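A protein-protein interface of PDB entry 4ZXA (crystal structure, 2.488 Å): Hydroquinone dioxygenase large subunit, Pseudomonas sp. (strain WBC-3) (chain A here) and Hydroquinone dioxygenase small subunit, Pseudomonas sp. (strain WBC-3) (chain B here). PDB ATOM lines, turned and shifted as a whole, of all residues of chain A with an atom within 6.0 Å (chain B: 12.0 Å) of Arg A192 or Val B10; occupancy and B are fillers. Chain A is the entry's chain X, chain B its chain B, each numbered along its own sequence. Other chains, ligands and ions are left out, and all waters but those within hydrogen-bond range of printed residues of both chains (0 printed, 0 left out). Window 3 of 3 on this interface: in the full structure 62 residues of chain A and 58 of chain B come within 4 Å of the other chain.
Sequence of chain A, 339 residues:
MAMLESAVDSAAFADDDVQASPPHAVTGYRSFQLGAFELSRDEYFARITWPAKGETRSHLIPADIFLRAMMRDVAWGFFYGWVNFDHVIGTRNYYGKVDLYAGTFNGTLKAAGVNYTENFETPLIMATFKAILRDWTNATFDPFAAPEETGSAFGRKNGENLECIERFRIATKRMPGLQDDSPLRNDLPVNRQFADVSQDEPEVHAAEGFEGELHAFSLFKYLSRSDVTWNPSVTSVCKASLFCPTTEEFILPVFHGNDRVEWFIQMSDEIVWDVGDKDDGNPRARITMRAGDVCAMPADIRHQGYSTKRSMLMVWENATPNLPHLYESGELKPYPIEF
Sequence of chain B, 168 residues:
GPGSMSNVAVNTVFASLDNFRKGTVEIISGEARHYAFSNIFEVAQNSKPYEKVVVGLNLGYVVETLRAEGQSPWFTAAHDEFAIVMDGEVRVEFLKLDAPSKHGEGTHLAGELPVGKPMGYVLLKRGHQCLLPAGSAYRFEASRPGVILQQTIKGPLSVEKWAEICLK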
ATOM      1  N   ALA A 146      15.636  16.200  -4.606  1.00  0.00           N
ATOM      2  CA  ALA A 146      15.953  14.824  -4.931  1.00  0.00           C
ATOM      3  C   ALA A 146      14.724  13.920  -4.694  1.00  0.00           C
ATOM      4  O   ALA A 146      13.796  14.293  -3.966  1.00  0.00           O
ATOM      5  CB  ALA A 146      17.146  14.363  -4.101  1.00  0.00           C
ATOM      6  N   GLU A 148      14.354  11.270  -2.997  1.00  0.00           N
ATOM      7  CA  GLU A 148      14.238  10.902  -1.588  1.00  0.00           C
ATOM      8  C   GLU A 148      13.712  12.037  -0.704  1.00  0.00           C
ATOM      9  O   GLU A 148      13.361  11.811   0.453  1.00  0.00           O
ATOM     10  CB  GLU A 148      15.585  10.427  -1.035  1.00  0.00           C
ATOM     11  CG  GLU A 148      16.000   9.032  -1.463  1.00  0.00           C
ATOM     12  CD  GLU A 148      17.341   8.614  -0.845  1.00  0.00           C
ATOM     13  OE1 GLU A 148      18.265   8.248  -1.605  1.00  0.00           O
ATOM     14  OE2 GLU A 148      17.482   8.650   0.400  1.00  0.00           O
ATOM     15  N   GLU A 149      13.667  13.254  -1.240  1.00  0.00           N
ATOM     16  CA  GLU A 149      13.277  14.416  -0.446  1.00  0.00           C
ATOM     17  C   GLU A 149      11.826  14.823  -0.682  1.00  0.00           C
ATOM     18  O   GLU A 149      11.336  15.794  -0.098  1.00  0.00           O
ATOM     19  CB  GLU A 149      14.158  15.613  -0.778  1.00  0.00           C
ATOM     20  CG  GLU A 149      15.639  15.412  -0.571  1.00  0.00           C
ATOM     21  CD  GLU A 149      16.387  16.730  -0.711  1.00  0.00           C
ATOM     22  OE1 GLU A 149      16.626  17.162  -1.859  1.00  0.00           O
ATOM     23  OE2 GLU A 149      16.705  17.353   0.327  1.00  0.00           O
ATOM     24  N   VAL A 190      20.207  22.634   7.813  1.00  0.00           N
ATOM     25  CA  VAL A 190      21.236  21.831   7.190  1.00  0.00           C
ATOM     26  C   VAL A 190      20.591  20.601   6.549  1.00  0.00           C
ATOM     27  O   VAL A 190      19.841  19.866   7.203  1.00  0.00           O
ATOM     28  CB  VAL A 190      22.267  21.385   8.230  1.00  0.00           C
ATOM     29  CG1 VAL A 190      23.237  20.372   7.622  1.00  0.00           C
ATOM     30  CG2 VAL A 190      23.004  22.605   8.797  1.00  0.00           C
ATOM     31  N   ASN A 191      20.863  20.392   5.263  1.00  0.00           N
ATOM     32  CA  ASN A 191      20.332  19.236   4.554  1.00  0.00           C
ATOM     33  C   ASN A 191      20.852  17.936   5.158  1.00  0.00           C
ATOM     34  O   ASN A 191      22.041  17.838   5.508  1.00  0.00           O
ATOM     35  CB  ASN A 191      20.717  19.304   3.086  1.00  0.00           C
ATOM     36  CG  ASN A 191      20.046  18.239   2.273  1.00  0.00           C
ATOM     37  OD1 ASN A 191      20.476  17.088   2.270  1.00  0.00           O
ATOM     38  ND2 ASN A 191      18.970  18.612   1.579  1.00  0.00           N
ATOM     39  N   ARG A 192      19.973  16.943   5.281  1.00  0.00           N
ATOM     40  CA  ARG A 192      20.337  15.688   5.935  1.00  0.00           C
ATOM     41  C   ARG A 192      21.646  15.096   5.433  1.00  0.00           C
ATOM     42  O   ARG A 192      22.388  14.518   6.215  1.00  0.00           O
ATOM     43  CB  ARG A 192      19.220  14.637   5.821  1.00  0.00           C
ATOM     44  CG  ARG A 192      19.169  13.863   4.485  1.00  0.00           C
ATOM     45  CD  ARG A 192      18.292  14.543   3.421  1.00  0.00           C
ATOM     46  NE  ARG A 192      17.949  13.607   2.344  1.00  0.00           N
ATOM     47  CZ  ARG A 192      18.422  13.669   1.098  1.00  0.00           C
ATOM     48  NH1 ARG A 192      19.250  14.646   0.726  1.00  0.00           N
ATOM     49  NH2 ARG A 192      18.050  12.756   0.216  1.00  0.00           N
ATOM     50  N   GLN A 193      21.933  15.230   4.140  1.00  0.00           N
ATOM     51  CA  GLN A 193      23.123  14.598   3.578  1.00  0.00           C
ATOM     52  C   GLN A 193      24.373  15.471   3.670  1.00  0.00           C
ATOM     53  O   GLN A 193      25.412  15.145   3.073  1.00  0.00           O
ATOM     54  CB  GLN A 193      22.899  14.151   2.131  1.00  0.00           C
ATOM     55  CG  GLN A 193      21.789  13.135   1.955  1.00  0.00           C
ATOM     56  CD  GLN A 193      21.959  12.297   0.694  1.00  0.00           C
ATOM     57  OE1 GLN A 193      22.757  12.632  -0.191  1.00  0.00           O
ATOM     58  NE2 GLN A 193      21.222  11.192   0.616  1.00  0.00           N
ATOM     59  N   PHE A 194      24.272  16.572   4.411  1.00  0.00           N
ATOM     60  CA  PHE A 194      25.442  17.394   4.737  1.00  0.00           C
ATOM     61  C   PHE A 194      25.499  17.612   6.236  1.00  0.00           C
ATOM     62  O   PHE A 194      26.187  18.524   6.708  1.00  0.00           O
ATOM     63  CB  PHE A 194      25.404  18.756   4.035  1.00  0.00           C
ATOM     64  CG  PHE A 194      25.726  18.699   2.572  1.00  0.00           C
ATOM     65  CD1 PHE A 194      26.810  17.974   2.115  1.00  0.00           C
ATOM     66  CD2 PHE A 194      24.939  19.377   1.654  1.00  0.00           C
ATOM     67  CE1 PHE A 194      27.107  17.927   0.773  1.00  0.00           C
ATOM     68  CE2 PHE A 194      25.222  19.326   0.310  1.00  0.00           C
ATOM     69  CZ  PHE A 194      26.309  18.600  -0.135  1.00  0.00           C
ATOM     70  N   ALA A 195      24.769  16.781   6.979  1.00  0.00           N
ATOM     71  CA  ALA A 195      24.694  16.908   8.442  1.00  0.00           C
ATOM     72  C   ALA A 195      26.047  16.914   9.159  1.00  0.00           C
ATOM     73  O   ALA A 195      26.131  17.369  10.305  1.00  0.00           O
ATOM     74  CB  ALA A 195      23.791  15.830   9.036  1.00  0.00           C
ATOM     75  N   ASP A 196      27.096  16.428   8.493  1.00  0.00           N
ATOM     76  CA  ASP A 196      28.423  16.368   9.097  1.00  0.00           C
ATOM     77  C   ASP A 196      29.340  17.515   8.653  1.00  0.00           C
ATOM     78  O   ASP A 196      30.545  17.510   8.946  1.00  0.00           O
ATOM     79  CB  ASP A 196      29.099  15.043   8.762  1.00  0.00           C
ATOM     80  CG  ASP A 196      29.431  14.917   7.279  1.00  0.00           C
ATOM     81  OD1 ASP A 196      28.557  15.255   6.448  1.00  0.00           O
ATOM     82  OD2 ASP A 196      30.564  14.498   6.943  1.00  0.00           O
ATOM     83  N   GLU A 249      22.307  15.981  -6.438  1.00  0.00           N
ATOM     84  CA  GLU A 249      21.843  14.689  -5.963  1.00  0.00           C
ATOM     85  C   GLU A 249      21.118  13.998  -7.103  1.00  0.00           C
ATOM     86  O   GLU A 249      20.520  14.656  -7.947  1.00  0.00           O
ATOM     87  CB  GLU A 249      20.928  14.846  -4.752  1.00  0.00           C
ATOM     88  CG  GLU A 249      20.842  13.613  -3.882  1.00  0.00           C
ATOM     89  CD  GLU A 249      20.022  13.840  -2.634  1.00  0.00           C
ATOM     90  OE1 GLU A 249      20.034  14.970  -2.110  1.00  0.00           O
ATOM     91  OE2 GLU A 249      19.366  12.890  -2.176  1.00  0.00           O
ATOM     92  N   LYS A 309      25.532  10.677  -3.662  1.00  0.00           N
ATOM     93  CA  LYS A 309      25.309  11.440  -2.450  1.00  0.00           C
ATOM     94  C   LYS A 309      25.214  12.902  -2.841  1.00  0.00           C
ATOM     95  O   LYS A 309      25.904  13.340  -3.757  1.00  0.00           O
ATOM     96  CB  LYS A 309      26.470  11.236  -1.475  1.00  0.00           C
ATOM     97  CG  LYS A 309      26.399  12.123  -0.262  1.00  0.00           C
ATOM     98  CD  LYS A 309      27.578  11.908   0.669  1.00  0.00           C
ATOM     99  CE  LYS A 309      27.568  12.943   1.768  1.00  0.00           C
ATOM    100  NZ  LYS A 309      27.806  14.299   1.200  1.00  0.00           N
ATOM    101  N   ARG A 310      24.350  13.654  -2.171  1.00  0.00           N
ATOM    102  CA  ARG A 310      24.311  15.097  -2.380  1.00  0.00           C
ATOM    103  C   ARG A 310      25.743  15.668  -2.298  1.00  0.00           C
ATOM    104  O   ARG A 310      26.410  15.607  -1.264  1.00  0.00           O
ATOM    105  CB  ARG A 310      23.407  15.741  -1.342  1.00  0.00           C
ATOM    106  CG  ARG A 310      22.996  17.172  -1.627  1.00  0.00           C
ATOM    107  CD  ARG A 310      22.120  17.657  -0.485  1.00  0.00           C
ATOM    108  NE  ARG A 310      21.285  18.788  -0.843  1.00  0.00           N
ATOM    109  CZ  ARG A 310      20.072  18.672  -1.377  1.00  0.00           C
ATOM    110  NH1 ARG A 310      19.569  17.466  -1.635  1.00  0.00           N
ATOM    111  NH2 ARG A 310      19.369  19.758  -1.660  1.00  0.00           N
ATOM    112  N   SER B   6      21.325  -0.787   8.694  1.00  0.00           N
ATOM    113  CA  SER B   6      22.591  -0.988   9.394  1.00  0.00           C
ATOM    114  C   SER B   6      23.382   0.329   9.535  1.00  0.00           C
ATOM    115  O   SER B   6      23.519   0.862  10.641  1.00  0.00           O
ATOM    116  CB  SER B   6      23.432  -2.075   8.700  1.00  0.00           C
ATOM    117  OG  SER B   6      23.990  -2.995   9.634  1.00  0.00           O
ATOM    118  N   ASN B   7      23.895   0.856   8.424  1.00  0.00           N
ATOM    119  CA  ASN B   7      24.622   2.127   8.464  1.00  0.00           C
ATOM    120  C   ASN B   7      23.741   3.342   8.171  1.00  0.00           C
ATOM    121  O   ASN B   7      22.973   3.359   7.199  1.00  0.00           O
ATOM    122  CB  ASN B   7      25.824   2.113   7.522  1.00  0.00           C
ATOM    123  CG  ASN B   7      26.907   3.087   7.953  1.00  0.00           C
ATOM    124  OD1 ASN B   7      26.637   4.058   8.668  1.00  0.00           O
ATOM    125  ND2 ASN B   7      28.142   2.830   7.525  1.00  0.00           N
ATOM    126  N   VAL B   8      23.856   4.354   9.024  1.00  0.00           N
ATOM    127  CA  VAL B   8      23.068   5.569   8.882  1.00  0.00           C
ATOM    128  C   VAL B   8      23.986   6.787   8.990  1.00  0.00           C
ATOM    129  O   VAL B   8      23.531   7.926   9.039  1.00  0.00           O
ATOM    130  CB  VAL B   8      21.955   5.618   9.930  1.00  0.00           C
ATOM    131  CG1 VAL B   8      20.987   6.765   9.639  1.00  0.00           C
ATOM    132  CG2 VAL B   8      21.219   4.277   9.953  1.00  0.00           C
ATOM    133  N   ALA B   9      25.290   6.533   8.995  1.00  0.00           N
ATOM    134  CA  ALA B   9      26.273   7.605   9.048  1.00  0.00           C
ATOM    135  C   ALA B   9      26.235   8.434   7.772  1.00  0.00           C
ATOM    136  O   ALA B   9      25.779   7.966   6.724  1.00  0.00           O
ATOM    137  CB  ALA B   9      27.673   7.040   9.272  1.00  0.00           C
ATOM    138  N   VAL B  10      26.718   9.668   7.874  1.00  0.00           N
ATOM    139  CA  VAL B  10      26.802  10.568   6.737  1.00  0.00           C
ATOM    140  C   VAL B  10      28.208  11.121   6.650  1.00  0.00           C
ATOM    141  O   VAL B  10      28.652  11.849   7.543  1.00  0.00           O
ATOM    142  CB  VAL B  10      25.839  11.744   6.892  1.00  0.00           C
ATOM    143  CG1 VAL B  10      25.936  12.666   5.685  1.00  0.00           C
ATOM    144  CG2 VAL B  10      24.434  11.236   7.058  1.00  0.00           C
ATOM    145  N   ASN B  11      28.910  10.785   5.574  1.00  0.00           N
ATOM    146  CA  ASN B  11      30.291  11.212   5.420  1.00  0.00           C
ATOM    147  C   ASN B  11      30.546  11.987   4.140  1.00  0.00           C
ATOM    148  O   ASN B  11      30.857  11.401   3.092  1.00  0.00           O
ATOM    149  CB  ASN B  11      31.234  10.018   5.538  1.00  0.00           C
ATOM    150  CG  ASN B  11      31.214   9.406   6.928  1.00  0.00           C
ATOM    151  OD1 ASN B  11      31.730   9.994   7.889  1.00  0.00           O
ATOM    152  ND2 ASN B  11      30.606   8.226   7.050  1.00  0.00           N
ATOM    153  N   THR B  12      30.402  13.306   4.234  1.00  0.00           N
ATOM    154  CA  THR B  12      30.722  14.212   3.139  1.00  0.00           C
ATOM    155  C   THR B  12      32.227  14.213   2.897  1.00  0.00           C
ATOM    156  O   THR B  12      32.997  14.706   3.719  1.00  0.00           O
ATOM    157  CB  THR B  12      30.275  15.632   3.476  1.00  0.00           C
ATOM    158  OG1 THR B  12      28.858  15.646   3.673  1.00  0.00           O
ATOM    159  CG2 THR B  12      30.662  16.615   2.369  1.00  0.00           C
ATOM    160  N   VAL B  13      32.643  13.659   1.765  1.00  0.00           N
ATOM    161  CA  VAL B  13      34.060  13.474   1.462  1.00  0.00           C
ATOM    162  C   VAL B  13      34.696  14.735   0.901  1.00  0.00           C
ATOM    163  O   VAL B  13      34.353  15.168  -0.202  1.00  0.00           O
ATOM    164  CB  VAL B  13      34.249  12.352   0.424  1.00  0.00           C
ATOM    165  CG1 VAL B  13      35.735  12.084   0.168  1.00  0.00           C
ATOM    166  CG2 VAL B  13      33.526  11.085   0.880  1.00  0.00           C
ATOM    167  N   PHE B  14      35.616  15.321   1.667  1.00  0.00           N
ATOM    168  CA  PHE B  14      36.471  16.416   1.197  1.00  0.00           C
ATOM    169  C   PHE B  14      37.883  15.891   1.052  1.00  0.00           C
ATOM    170  O   PHE B  14      38.285  14.977   1.773  1.00  0.00           O
ATOM    171  CB  PHE B  14      36.499  17.564   2.199  1.00  0.00           C
ATOM    172  CG  PHE B  14      35.176  18.252   2.383  1.00  0.00           C
ATOM    173  CD1 PHE B  14      34.634  19.025   1.366  1.00  0.00           C
ATOM    174  CD2 PHE B  14      34.490  18.155   3.584  1.00  0.00           C
ATOM    175  CE1 PHE B  14      33.425  19.680   1.536  1.00  0.00           C
ATOM    176  CE2 PHE B  14      33.277  18.806   3.760  1.00  0.00           C
ATOM    177  CZ  PHE B  14      32.745  19.568   2.733  1.00  0.00           C
ATOM    178  N   ARG B 126      39.056  25.707   6.042  1.00  0.00           N
ATOM    179  CA  ARG B 126      38.502  25.002   4.900  1.00  0.00           C
ATOM    180  C   ARG B 126      37.040  25.369   4.650  1.00  0.00           C
ATOM    181  O   ARG B 126      36.237  25.452   5.585  1.00  0.00           O
ATOM    182  CB  ARG B 126      38.610  23.498   5.109  1.00  0.00           C
ATOM    183  CG  ARG B 126      37.861  22.692   4.067  1.00  0.00           C
ATOM    184  CD  ARG B 126      38.226  21.237   4.180  1.00  0.00           C
ATOM    185  NE  ARG B 126      37.402  20.552   5.162  1.00  0.00           N
ATOM    186  CZ  ARG B 126      37.645  19.319   5.584  1.00  0.00           C
ATOM    187  NH1 ARG B 126      38.706  18.664   5.118  1.00  0.00           N
ATOM    188  NH2 ARG B 126      36.832  18.742   6.463  1.00  0.00           N
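Among the printed residues, merely in contact across the chains: Phe A194 with Thr B12 (3.5 Å), Gln A193 with Thr B12 (3.5 Å), Asp A196 with Asn B11 (3.6 Å), Gln A193 with Val B10 (3.6 Å), Lys A309 with Asn B11 (3.9 Å) and Arg A192 with Val B10 (3.96 Å).
Of the 13 printed residues of chain A, 5 touch a printed residue of chain B. Printed residues of chain A that touch a printed residue of chain B: Arg A192, Gln A193, Phe A194, Asp A196 and Lys A309. Hydrophobic or aromatic side chains of chain A within 4 Å of the printed part of chain B: Phe A194. Among the printed residues, 9 pairs touch across the chains.
OE2 of Glu A149 lies within salt-bridge range of NH1 of Arg A192. The side-chain amide oxygen (OD1) of Asn A191 is in hydrogen-bond range of the guanidinium group (NH1) of Arg A192, 3.1 Å away. N of Gln A193 sits at hydrogen-bond distance from OD1 of Asn A191 (3.0 Å). NH2 of Arg A192 is in salt-bridge range of OE2 of Glu A249 (2.7 Å). The backbone carbonyl oxygen (O) of Gln A193 lies within hydrogen-bond range of the side-chain amino group (NZ) of Lys A309 (3.2 Å). OE1 of Gln A193 lies within hydrogen-bond range of N of Arg A310 (2.7 Å).
Arg A192 touches just one residue of chain B: Val B10. Val B10 touches just these residues of chain A: Arg A192, Gln A193 and Asp A196. No residue of chain B comes within 4 Å of Ala A146. No residue of chain B comes within 4 Å of Glu A148. No residue of chain B comes within 4 Å of Glu A149. No residue of chain B comes within 4 Å of Val A190. No residue of chain B comes within 4 Å of Asn A191. Gln A193 touches just these residues of chain B: Val B10 (3.6 Å) and Thr B12 (3.5 Å). Of chain B, only Val B10, Asn B11 and Thr B12 come within 4 Å of Asp A196. No residue of chain B comes within 4 Å of Arg A310. Printed residues of chain B within 4 Å of Lys A309: Asn B11 (3.9 Å) and Thr B12 (3.0 Å). Printed residues of chain B within 4 Å of Phe A194: Thr B12 (3.5 Å). The nearest residue of chain A that does not touch Val B10 is Lys A309 (4.3 Å).
The side-chain hydroxyl (OG1) of Thr B12 is in hydrogen-bond range of the side-chain carboxylate (OD1) of Asp A196. NZ of Lys A309 is in hydrogen-bond range of OG1 of Thr B12 (3.0 Å). The side-chain carboxylate (OD2) of Asp A196 sits close to the backbone carbonyl oxygen (O) of Val B10 (3.3 Å).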
